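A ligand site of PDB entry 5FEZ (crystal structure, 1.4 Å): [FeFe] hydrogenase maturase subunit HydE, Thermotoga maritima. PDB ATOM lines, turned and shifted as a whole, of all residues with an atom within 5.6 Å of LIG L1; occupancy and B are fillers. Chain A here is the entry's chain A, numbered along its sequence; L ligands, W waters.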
ATOM      1  N   CYS A  73     -24.690  19.732  21.524  1.00  0.00           N
ATOM      2  CA  CYS A  73     -24.643  21.091  22.077  1.00  0.00           C
ATOM      3  C   CYS A  73     -24.754  21.144  23.582  1.00  0.00           C
ATOM      4  O   CYS A  73     -25.496  20.400  24.176  1.00  0.00           O
ATOM      5  CB  CYS A  73     -25.785  21.983  21.528  1.00  0.00           C
ATOM      6  SG  CYS A  73     -25.388  23.754  21.846  1.00  0.00           S
ATOM      7  N   CYS A  80     -34.417  25.884  19.715  1.00  0.00           N
ATOM      8  CA  CYS A  80     -33.559  25.054  18.886  1.00  0.00           C
ATOM      9  C   CYS A  80     -33.703  23.562  19.059  1.00  0.00           C
ATOM     10  O   CYS A  80     -33.604  23.073  20.190  1.00  0.00           O
ATOM     11  CB  CYS A  80     -32.111  25.415  19.150  1.00  0.00           C
ATOM     12  SG  CYS A  80     -30.882  24.557  18.116  1.00  0.00           S
ATOM     13  N   LEU A  82     -31.582  21.280  18.602  1.00  0.00           N
ATOM     14  CA  LEU A  82     -30.380  20.700  19.125  1.00  0.00           C
ATOM     15  C   LEU A  82     -30.140  20.983  20.612  1.00  0.00           C
ATOM     16  O   LEU A  82     -29.163  20.511  21.165  1.00  0.00           O
ATOM     17  CB  LEU A  82     -29.124  21.119  18.332  1.00  0.00           C
ATOM     18  CG  LEU A  82     -29.155  20.870  16.851  1.00  0.00           C
ATOM     19  CD1 LEU A  82     -27.805  21.159  16.244  1.00  0.00           C
ATOM     20  CD2 LEU A  82     -29.750  19.642  16.352  1.00  0.00           C
ATOM     21  N   GLN A 117     -20.187  24.368  10.643  1.00  0.00           N
ATOM     22  CA  GLN A 117     -21.168  24.713  11.640  1.00  0.00           C
ATOM     23  C   GLN A 117     -21.393  23.543  12.546  1.00  0.00           C
ATOM     24  O   GLN A 117     -21.423  22.394  12.114  1.00  0.00           O
ATOM     25  CB  GLN A 117     -22.500  25.218  11.018  1.00  0.00           C
ATOM     26  CG  GLN A 117     -23.446  25.823  12.062  1.00  0.00           C
ATOM     27  CD  GLN A 117     -24.740  26.268  11.463  1.00  0.00           C
ATOM     28  OE1 GLN A 117     -25.641  25.450  11.289  1.00  0.00           O
ATOM     29  NE2 GLN A 117     -24.864  27.508  11.168  1.00  0.00           N
ATOM     30  N   SER A 118     -21.665  23.826  13.818  1.00  0.00           N
ATOM     31  CA  SER A 118     -21.996  22.773  14.771  1.00  0.00           C
ATOM     32  C   SER A 118     -22.800  23.338  15.909  1.00  0.00           C
ATOM     33  O   SER A 118     -22.862  24.562  16.130  1.00  0.00           O
ATOM     34  CB  SER A 118     -20.714  22.099  15.298  1.00  0.00           C
ATOM     35  OG  SER A 118     -19.892  23.009  15.989  1.00  0.00           O
ATOM     36  N   GLY A 119     -23.349  22.437  16.703  1.00  0.00           N
ATOM     37  CA  GLY A 119     -23.711  22.777  18.079  1.00  0.00           C
ATOM     38  C   GLY A 119     -22.480  23.255  18.827  1.00  0.00           C
ATOM     39  O   GLY A 119     -21.321  23.049  18.377  1.00  0.00           O
ATOM     40  N   GLU A 120     -22.634  23.839  19.987  1.00  0.00           N
ATOM     41  CA  GLU A 120     -21.532  24.160  20.848  1.00  0.00           C
ATOM     42  C   GLU A 120     -21.018  22.868  21.493  1.00  0.00           C
ATOM     43  O   GLU A 120     -21.395  22.518  22.653  1.00  0.00           O
ATOM     44  CB  GLU A 120     -21.870  25.201  21.902  1.00  0.00           C
ATOM     45  CG  GLU A 120     -22.119  26.581  21.315  1.00  0.00           C
ATOM     46  CD  GLU A 120     -22.124  27.686  22.345  1.00  0.00           C
ATOM     47  OE1 GLU A 120     -21.851  27.401  23.533  1.00  0.00           O
ATOM     48  OE2 GLU A 120     -22.432  28.851  21.983  1.00  0.00           O
ATOM     49  N   SER A 146     -18.900  28.671  12.264  1.00  0.00           N
ATOM     50  CA  SER A 146     -20.191  28.993  12.939  1.00  0.00           C
ATOM     51  C   SER A 146     -20.341  27.999  14.093  1.00  0.00           C
ATOM     52  O   SER A 146     -21.079  27.056  14.017  1.00  0.00           O
ATOM     53  CB  SER A 146     -21.344  28.881  11.962  1.00  0.00           C
ATOM     54  OG  SER A 146     -22.555  29.337  12.518  1.00  0.00           O
ATOM     55  N   LEU A 147     -19.608  28.274  15.145  1.00  0.00           N
ATOM     56  CA  LEU A 147     -19.452  27.333  16.252  1.00  0.00           C
ATOM     57  C   LEU A 147     -20.019  27.860  17.543  1.00  0.00           C
ATOM     58  O   LEU A 147     -19.929  27.144  18.580  1.00  0.00           O
ATOM     59  CB  LEU A 147     -17.980  26.952  16.437  1.00  0.00           C
ATOM     60  CG  LEU A 147     -17.238  26.556  15.203  1.00  0.00           C
ATOM     61  CD1 LEU A 147     -15.788  26.235  15.511  1.00  0.00           C
ATOM     62  CD2 LEU A 147     -17.882  25.418  14.457  1.00  0.00           C
ATOM     63  N   GLY A 148     -20.594  29.058  17.568  1.00  0.00           N
ATOM     64  CA  GLY A 148     -21.158  29.591  18.815  1.00  0.00           C
ATOM     65  C   GLY A 148     -20.183  30.480  19.590  1.00  0.00           C
ATOM     66  O   GLY A 148     -19.234  31.030  19.053  1.00  0.00           O
ATOM     67  N   GLU A 149     -20.507  30.554  20.897  1.00  0.00           N
ATOM     68  CA  GLU A 149     -19.788  31.431  21.823  1.00  0.00           C
ATOM     69  C   GLU A 149     -18.673  30.665  22.540  1.00  0.00           C
ATOM     70  O   GLU A 149     -18.913  29.671  23.165  1.00  0.00           O
ATOM     71  CB  GLU A 149     -20.765  31.903  22.883  1.00  0.00           C
ATOM     72  CG  GLU A 149     -21.894  32.734  22.319  1.00  0.00           C
ATOM     73  CD  GLU A 149     -23.010  33.069  23.262  1.00  0.00           C
ATOM     74  OE1 GLU A 149     -22.724  33.266  24.488  1.00  0.00           O
ATOM     75  OE2 GLU A 149     -24.157  33.186  22.841  1.00  0.00           O
ATOM     76  N   LEU A 167     -19.700  33.323  11.586  1.00  0.00           N
ATOM     77  CA  LEU A 167     -21.135  33.622  11.652  1.00  0.00           C
ATOM     78  C   LEU A 167     -21.606  33.442  13.053  1.00  0.00           C
ATOM     79  O   LEU A 167     -21.476  32.369  13.583  1.00  0.00           O
ATOM     80  CB  LEU A 167     -21.928  32.675  10.769  1.00  0.00           C
ATOM     81  CG  LEU A 167     -21.470  32.542   9.312  1.00  0.00           C
ATOM     82  CD1 LEU A 167     -22.324  31.532   8.550  1.00  0.00           C
ATOM     83  CD2 LEU A 167     -21.459  33.875   8.643  1.00  0.00           C
ATOM     84  N   LEU A 168     -22.204  34.442  13.656  1.00  0.00           N
ATOM     85  CA  LEU A 168     -22.712  34.362  15.012  1.00  0.00           C
ATOM     86  C   LEU A 168     -23.957  35.243  15.042  1.00  0.00           C
ATOM     87  O   LEU A 168     -23.878  36.415  15.373  1.00  0.00           O
ATOM     88  CB  LEU A 168     -21.695  34.805  16.021  1.00  0.00           C
ATOM     89  CG  LEU A 168     -22.030  34.507  17.486  1.00  0.00           C
ATOM     90  CD1 LEU A 168     -21.943  33.033  17.765  1.00  0.00           C
ATOM     91  CD2 LEU A 168     -21.057  35.311  18.386  1.00  0.00           C
ATOM     92  N   ARG A 169     -25.092  34.719  14.659  1.00  0.00           N
ATOM     93  CA  ARG A 169     -26.282  35.532  14.634  1.00  0.00           C
ATOM     94  C   ARG A 169     -26.482  36.170  15.960  1.00  0.00           C
ATOM     95  O   ARG A 169     -26.361  35.510  16.989  1.00  0.00           O
ATOM     96  CB  ARG A 169     -27.475  34.722  14.258  1.00  0.00           C
ATOM     97  CG  ARG A 169     -27.484  34.321  12.772  1.00  0.00           C
ATOM     98  CD  ARG A 169     -28.803  33.678  12.546  1.00  0.00           C
ATOM     99  NE  ARG A 169     -28.913  33.204  11.195  1.00  0.00           N
ATOM    100  CZ  ARG A 169     -30.048  32.758  10.696  1.00  0.00           C
ATOM    101  NH1 ARG A 169     -31.181  32.687  11.434  1.00  0.00           N
ATOM    102  NH2 ARG A 169     -30.109  32.439   9.443  1.00  0.00           N
ATOM    103  N   GLU A 171     -29.413  36.926  17.055  1.00  0.00           N
ATOM    104  CA  GLU A 171     -30.692  36.285  17.367  1.00  0.00           C
ATOM    105  C   GLU A 171     -31.859  37.238  17.622  1.00  0.00           C
ATOM    106  O   GLU A 171     -32.863  37.194  16.971  1.00  0.00           O
ATOM    107  CB  GLU A 171     -30.547  35.239  18.487  1.00  0.00           C
ATOM    108  CG  GLU A 171     -29.379  34.255  18.333  1.00  0.00           C
ATOM    109  CD  GLU A 171     -29.480  33.369  17.127  1.00  0.00           C
ATOM    110  OE1 GLU A 171     -30.324  33.506  16.261  1.00  0.00           O
ATOM    111  OE2 GLU A 171     -28.609  32.493  17.032  1.00  0.00           O
ATOM    112  N   ARG A 182     -32.366  32.263  25.543  1.00  0.00           N
ATOM    113  CA  ARG A 182     -31.009  31.709  25.577  1.00  0.00           C
ATOM    114  C   ARG A 182     -30.472  31.796  27.029  1.00  0.00           C
ATOM    115  O   ARG A 182     -29.648  32.556  27.387  1.00  0.00           O
ATOM    116  CB  ARG A 182     -30.128  32.467  24.581  1.00  0.00           C
ATOM    117  CG  ARG A 182     -30.753  32.596  23.195  1.00  0.00           C
ATOM    118  CD  ARG A 182     -29.845  33.152  22.125  1.00  0.00           C
ATOM    119  NE  ARG A 182     -28.750  32.190  21.894  1.00  0.00           N
ATOM    120  CZ  ARG A 182     -27.506  32.341  22.215  1.00  0.00           C
ATOM    121  NH1 ARG A 182     -27.030  33.464  22.608  1.00  0.00           N
ATOM    122  NH2 ARG A 182     -26.699  31.276  22.071  1.00  0.00           N
ATOM    123  N   ARG A 190     -23.183  37.808  23.705  1.00  0.00           N
ATOM    124  CA  ARG A 190     -23.245  37.642  22.241  1.00  0.00           C
ATOM    125  C   ARG A 190     -22.574  38.771  21.516  1.00  0.00           C
ATOM    126  O   ARG A 190     -21.773  38.593  20.592  1.00  0.00           O
ATOM    127  CB  ARG A 190     -24.723  37.520  21.835  1.00  0.00           C
ATOM    128  CG  ARG A 190     -24.989  36.909  20.437  1.00  0.00           C
ATOM    129  CD  ARG A 190     -24.762  35.424  20.514  1.00  0.00           C
ATOM    130  NE  ARG A 190     -25.245  34.720  19.302  1.00  0.00           N
ATOM    131  CZ  ARG A 190     -25.074  33.405  19.102  1.00  0.00           C
ATOM    132  NH1 ARG A 190     -24.502  32.672  20.036  1.00  0.00           N
ATOM    133  NH2 ARG A 190     -25.466  32.896  17.969  1.00  0.00           N
ATOM    134  N   TYR A 313     -29.546  16.867  11.851  1.00  0.00           N
ATOM    135  CA  TYR A 313     -29.236  18.277  12.158  1.00  0.00           C
ATOM    136  C   TYR A 313     -30.434  19.117  11.788  1.00  0.00           C
ATOM    137  O   TYR A 313     -30.482  19.723  10.740  1.00  0.00           O
ATOM    138  CB  TYR A 313     -27.998  18.740  11.441  1.00  0.00           C
ATOM    139  CG  TYR A 313     -27.328  20.016  12.004  1.00  0.00           C
ATOM    140  CD1 TYR A 313     -26.285  19.959  12.881  1.00  0.00           C
ATOM    141  CD2 TYR A 313     -27.724  21.268  11.609  1.00  0.00           C
ATOM    142  CE1 TYR A 313     -25.643  21.068  13.328  1.00  0.00           C
ATOM    143  CE2 TYR A 313     -27.070  22.381  12.035  1.00  0.00           C
ATOM    144  CZ  TYR A 313     -26.050  22.283  12.845  1.00  0.00           C
ATOM    145  OH  TYR A 313     -25.286  23.338  13.278  1.00  0.00           O
ATOM    146  N   LEU A 315     -32.486  22.006  13.270  1.00  0.00           N
ATOM    147  CA  LEU A 315     -32.692  23.085  14.192  1.00  0.00           C
ATOM    148  C   LEU A 315     -34.188  23.360  14.271  1.00  0.00           C
ATOM    149  O   LEU A 315     -34.708  23.697  15.292  1.00  0.00           O
ATOM    150  CB  LEU A 315     -31.982  24.349  13.683  1.00  0.00           C
ATOM    151  CG  LEU A 315     -30.511  24.160  13.331  1.00  0.00           C
ATOM    152  CD1 LEU A 315     -29.899  25.467  12.891  1.00  0.00           C
ATOM    153  CD2 LEU A 315     -29.803  23.546  14.407  1.00  0.00           C
HETATM  154  N1  LIG L   1     -24.479  26.901  17.846  1.00  0.00           N
HETATM  155  C1  LIG L   1     -24.005  27.996  16.971  1.00  0.00           C
HETATM  156  C2  LIG L   1     -24.787  29.271  17.273  1.00  0.00           C
HETATM  157  O1  LIG L   1     -24.391  30.356  16.906  1.00  0.00           O
HETATM  158  C3  LIG L   1     -24.167  27.555  15.529  1.00  0.00           C
HETATM  159  C4  LIG L   1     -25.563  27.812  14.963  1.00  0.00           C
HETATM  160  S1  LIG L   1     -26.871  26.931  15.826  1.00  0.00           S
HETATM  161  C5  LIG L   1     -26.365  25.284  15.187  1.00  0.00           C
HETATM  162  O2  LIG L   1     -25.835  29.026  17.972  1.00  0.00           O
HETATM  163 SE1  LG2 L   2     -29.089  25.081  21.455  1.00  0.00          SE
HETATM  164 FE1  LG2 L   2     -28.997  25.395  19.045  1.00  0.00          FE
HETATM  165 FE2  LG2 L   2     -28.422  27.313  20.885  1.00  0.00          FE
HETATM  166 FE3  LG2 L   2     -26.878  25.065  20.692  1.00  0.00          FE
HETATM  167 SE2  LG2 L   2     -27.002  24.541  18.409  1.00  0.00          SE
HETATM  168 FE4  LG2 L   2     -26.644  26.971  18.444  1.00  0.00          FE
HETATM  169 SE3  LG2 L   2     -29.016  27.722  18.601  1.00  0.00          SE
HETATM  170 SE4  LG2 L   2     -26.067  27.287  20.941  1.00  0.00          SE
HETATM  171  N1  LG3 L   3     -36.283  28.245  13.664  1.00  0.00           N
HETATM  172  C1  LG3 L   3     -35.565  28.979  12.795  1.00  0.00           C
HETATM  173  N2  LG3 L   3     -34.253  29.243  12.920  1.00  0.00           N
HETATM  174  C2  LG3 L   3     -33.619  28.687  13.919  1.00  0.00           C
HETATM  175  N3  LG3 L   3     -32.356  28.708  14.274  1.00  0.00           N
HETATM  176  C3  LG3 L   3     -32.250  27.922  15.362  1.00  0.00           C
HETATM  177  N4  LG3 L   3     -33.391  27.390  15.688  1.00  0.00           N
HETATM  178  C4  LG3 L   3     -34.306  27.832  14.793  1.00  0.00           C
HETATM  179  C5  LG3 L   3     -35.695  27.634  14.634  1.00  0.00           C
HETATM  180  N5  LG3 L   3     -36.429  26.842  15.462  1.00  0.00           N
HETATM  181  C6  LG3 L   3     -31.367  29.611  13.702  1.00  0.00           C
HETATM  182  C7  LG3 L   3     -30.708  30.517  14.740  1.00  0.00           C
HETATM  183  C8  LG3 L   3     -29.259  30.124  14.636  1.00  0.00           C
HETATM  184  C9  LG3 L   3     -29.141  29.674  13.200  1.00  0.00           C
HETATM  185  C10 LG3 L   3     -28.069  28.648  13.008  1.00  0.00           C
HETATM  186  O1  LG3 L   3     -30.337  28.890  13.071  1.00  0.00           O
HETATM  187  O2  LG3 L   3     -30.943  31.874  14.333  1.00  0.00           O
HETATM  188  O3  LG3 L   3     -28.314  31.193  14.852  1.00  0.00           O
HETATM  189  O   HOH W   1     -28.149  30.828  19.140  1.00  0.00           O
HETATM  190  O   HOH W   2     -25.615  31.685  14.732  1.00  0.00           O
HETATM  191  O   HOH W   3     -24.212  29.927  20.304  1.00  0.00           O
HETATM  192  O   HOH W   4     -22.061  30.413  15.402  1.00  0.00           O
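A nitrogen (N1) of LIG L1 binds an iron atom (FE4) of LG2 L2 (2.2 Å).
The backbone carbonyl oxygen of Ser 118 lies close to a nitrogen (N1) of LIG L1, at 3.3 Å. The guanidinium group of Arg 169 sits at hydrogen-bond distance from an oxygen (O2) of LG3 L3 (3.0 Å). The guanidinium group (NH2) of Arg 190 lies within salt-bridge range of an oxygen (O1) of LIG L1 (3.0 Å). FE1 of LG2 L2 is bound by SG of Cys 80 (2.3 Å). The side-chain sulfur (SG) of Cys 73 is bound to an iron atom (FE3) of LG2 L2, at 2.3 Å. OE2 of Glu 171 sits at hydrogen-bond distance from O3 of LG3 L3 (2.6 Å).
Gln 117 touches LIG L1. Ser 146 touches LIG L1. Gly 148 touches LIG L1 (N to C1, 3.6 Å). Leu 168 touches LIG L1. Tyr 313 touches LIG L1 (OH to C5, 2.9 Å). Leu 315 touches LIG L1. Hydrophobic or aromatic side chains within 4 Å of LIG L1: Leu 168, Tyr 313 and Leu 315.
The side-chain carboxylate (OE2) of Glu 171 is in salt-bridge range of the guanidinium group (NH2) of Arg 190, 3.3 Å away. The backbone NH of Ser 118 lies within hydrogen-bond range of the backbone carbonyl oxygen of Ser 146, at 3.3 Å. The side-chain amide nitrogen (NE2) of Gln 117 is in hydrogen-bond range of the side-chain hydroxyl (OG) of Ser 146 (3.2 Å). OH of Tyr 313 lies within hydrogen-bond range of OE1 of Gln 117 (2.9 Å). The backbone carbonyl oxygen (O) of Arg 169 lies within hydrogen-bond range of the guanidinium group (NE) of Arg 190 (2.7 Å). O of Leu 167 sits at hydrogen-bond distance from OG of Ser 146 (3.4 Å). NH1 of Arg 190 lies within salt-bridge range of OE2 of Glu 149 (2.9 Å).
Water W4 lies within hydrogen-bond range of O of Leu 167, O1 of LIG L1, N of Gly 148, OG of Ser 146 and N of Leu 147. Water W2 lies within hydrogen-bond range of an oxygen (O3) of LG3 L3, an oxygen (O1) of LIG L1, the backbone NH of Arg 169 and the guanidinium group of Arg 190. Water W3 lies within hydrogen-bond range of the side-chain carboxylate of Glu 120 (2.7 Å), the guanidinium group of Arg 190 (2.8 Å), the guanidinium group of Arg 182 (3.3 Å) and an oxygen (O1) of LIG L1 (3.4 Å). Water W1 lies within hydrogen-bond range of OE2 of Glu 171 and NE of Arg 182.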
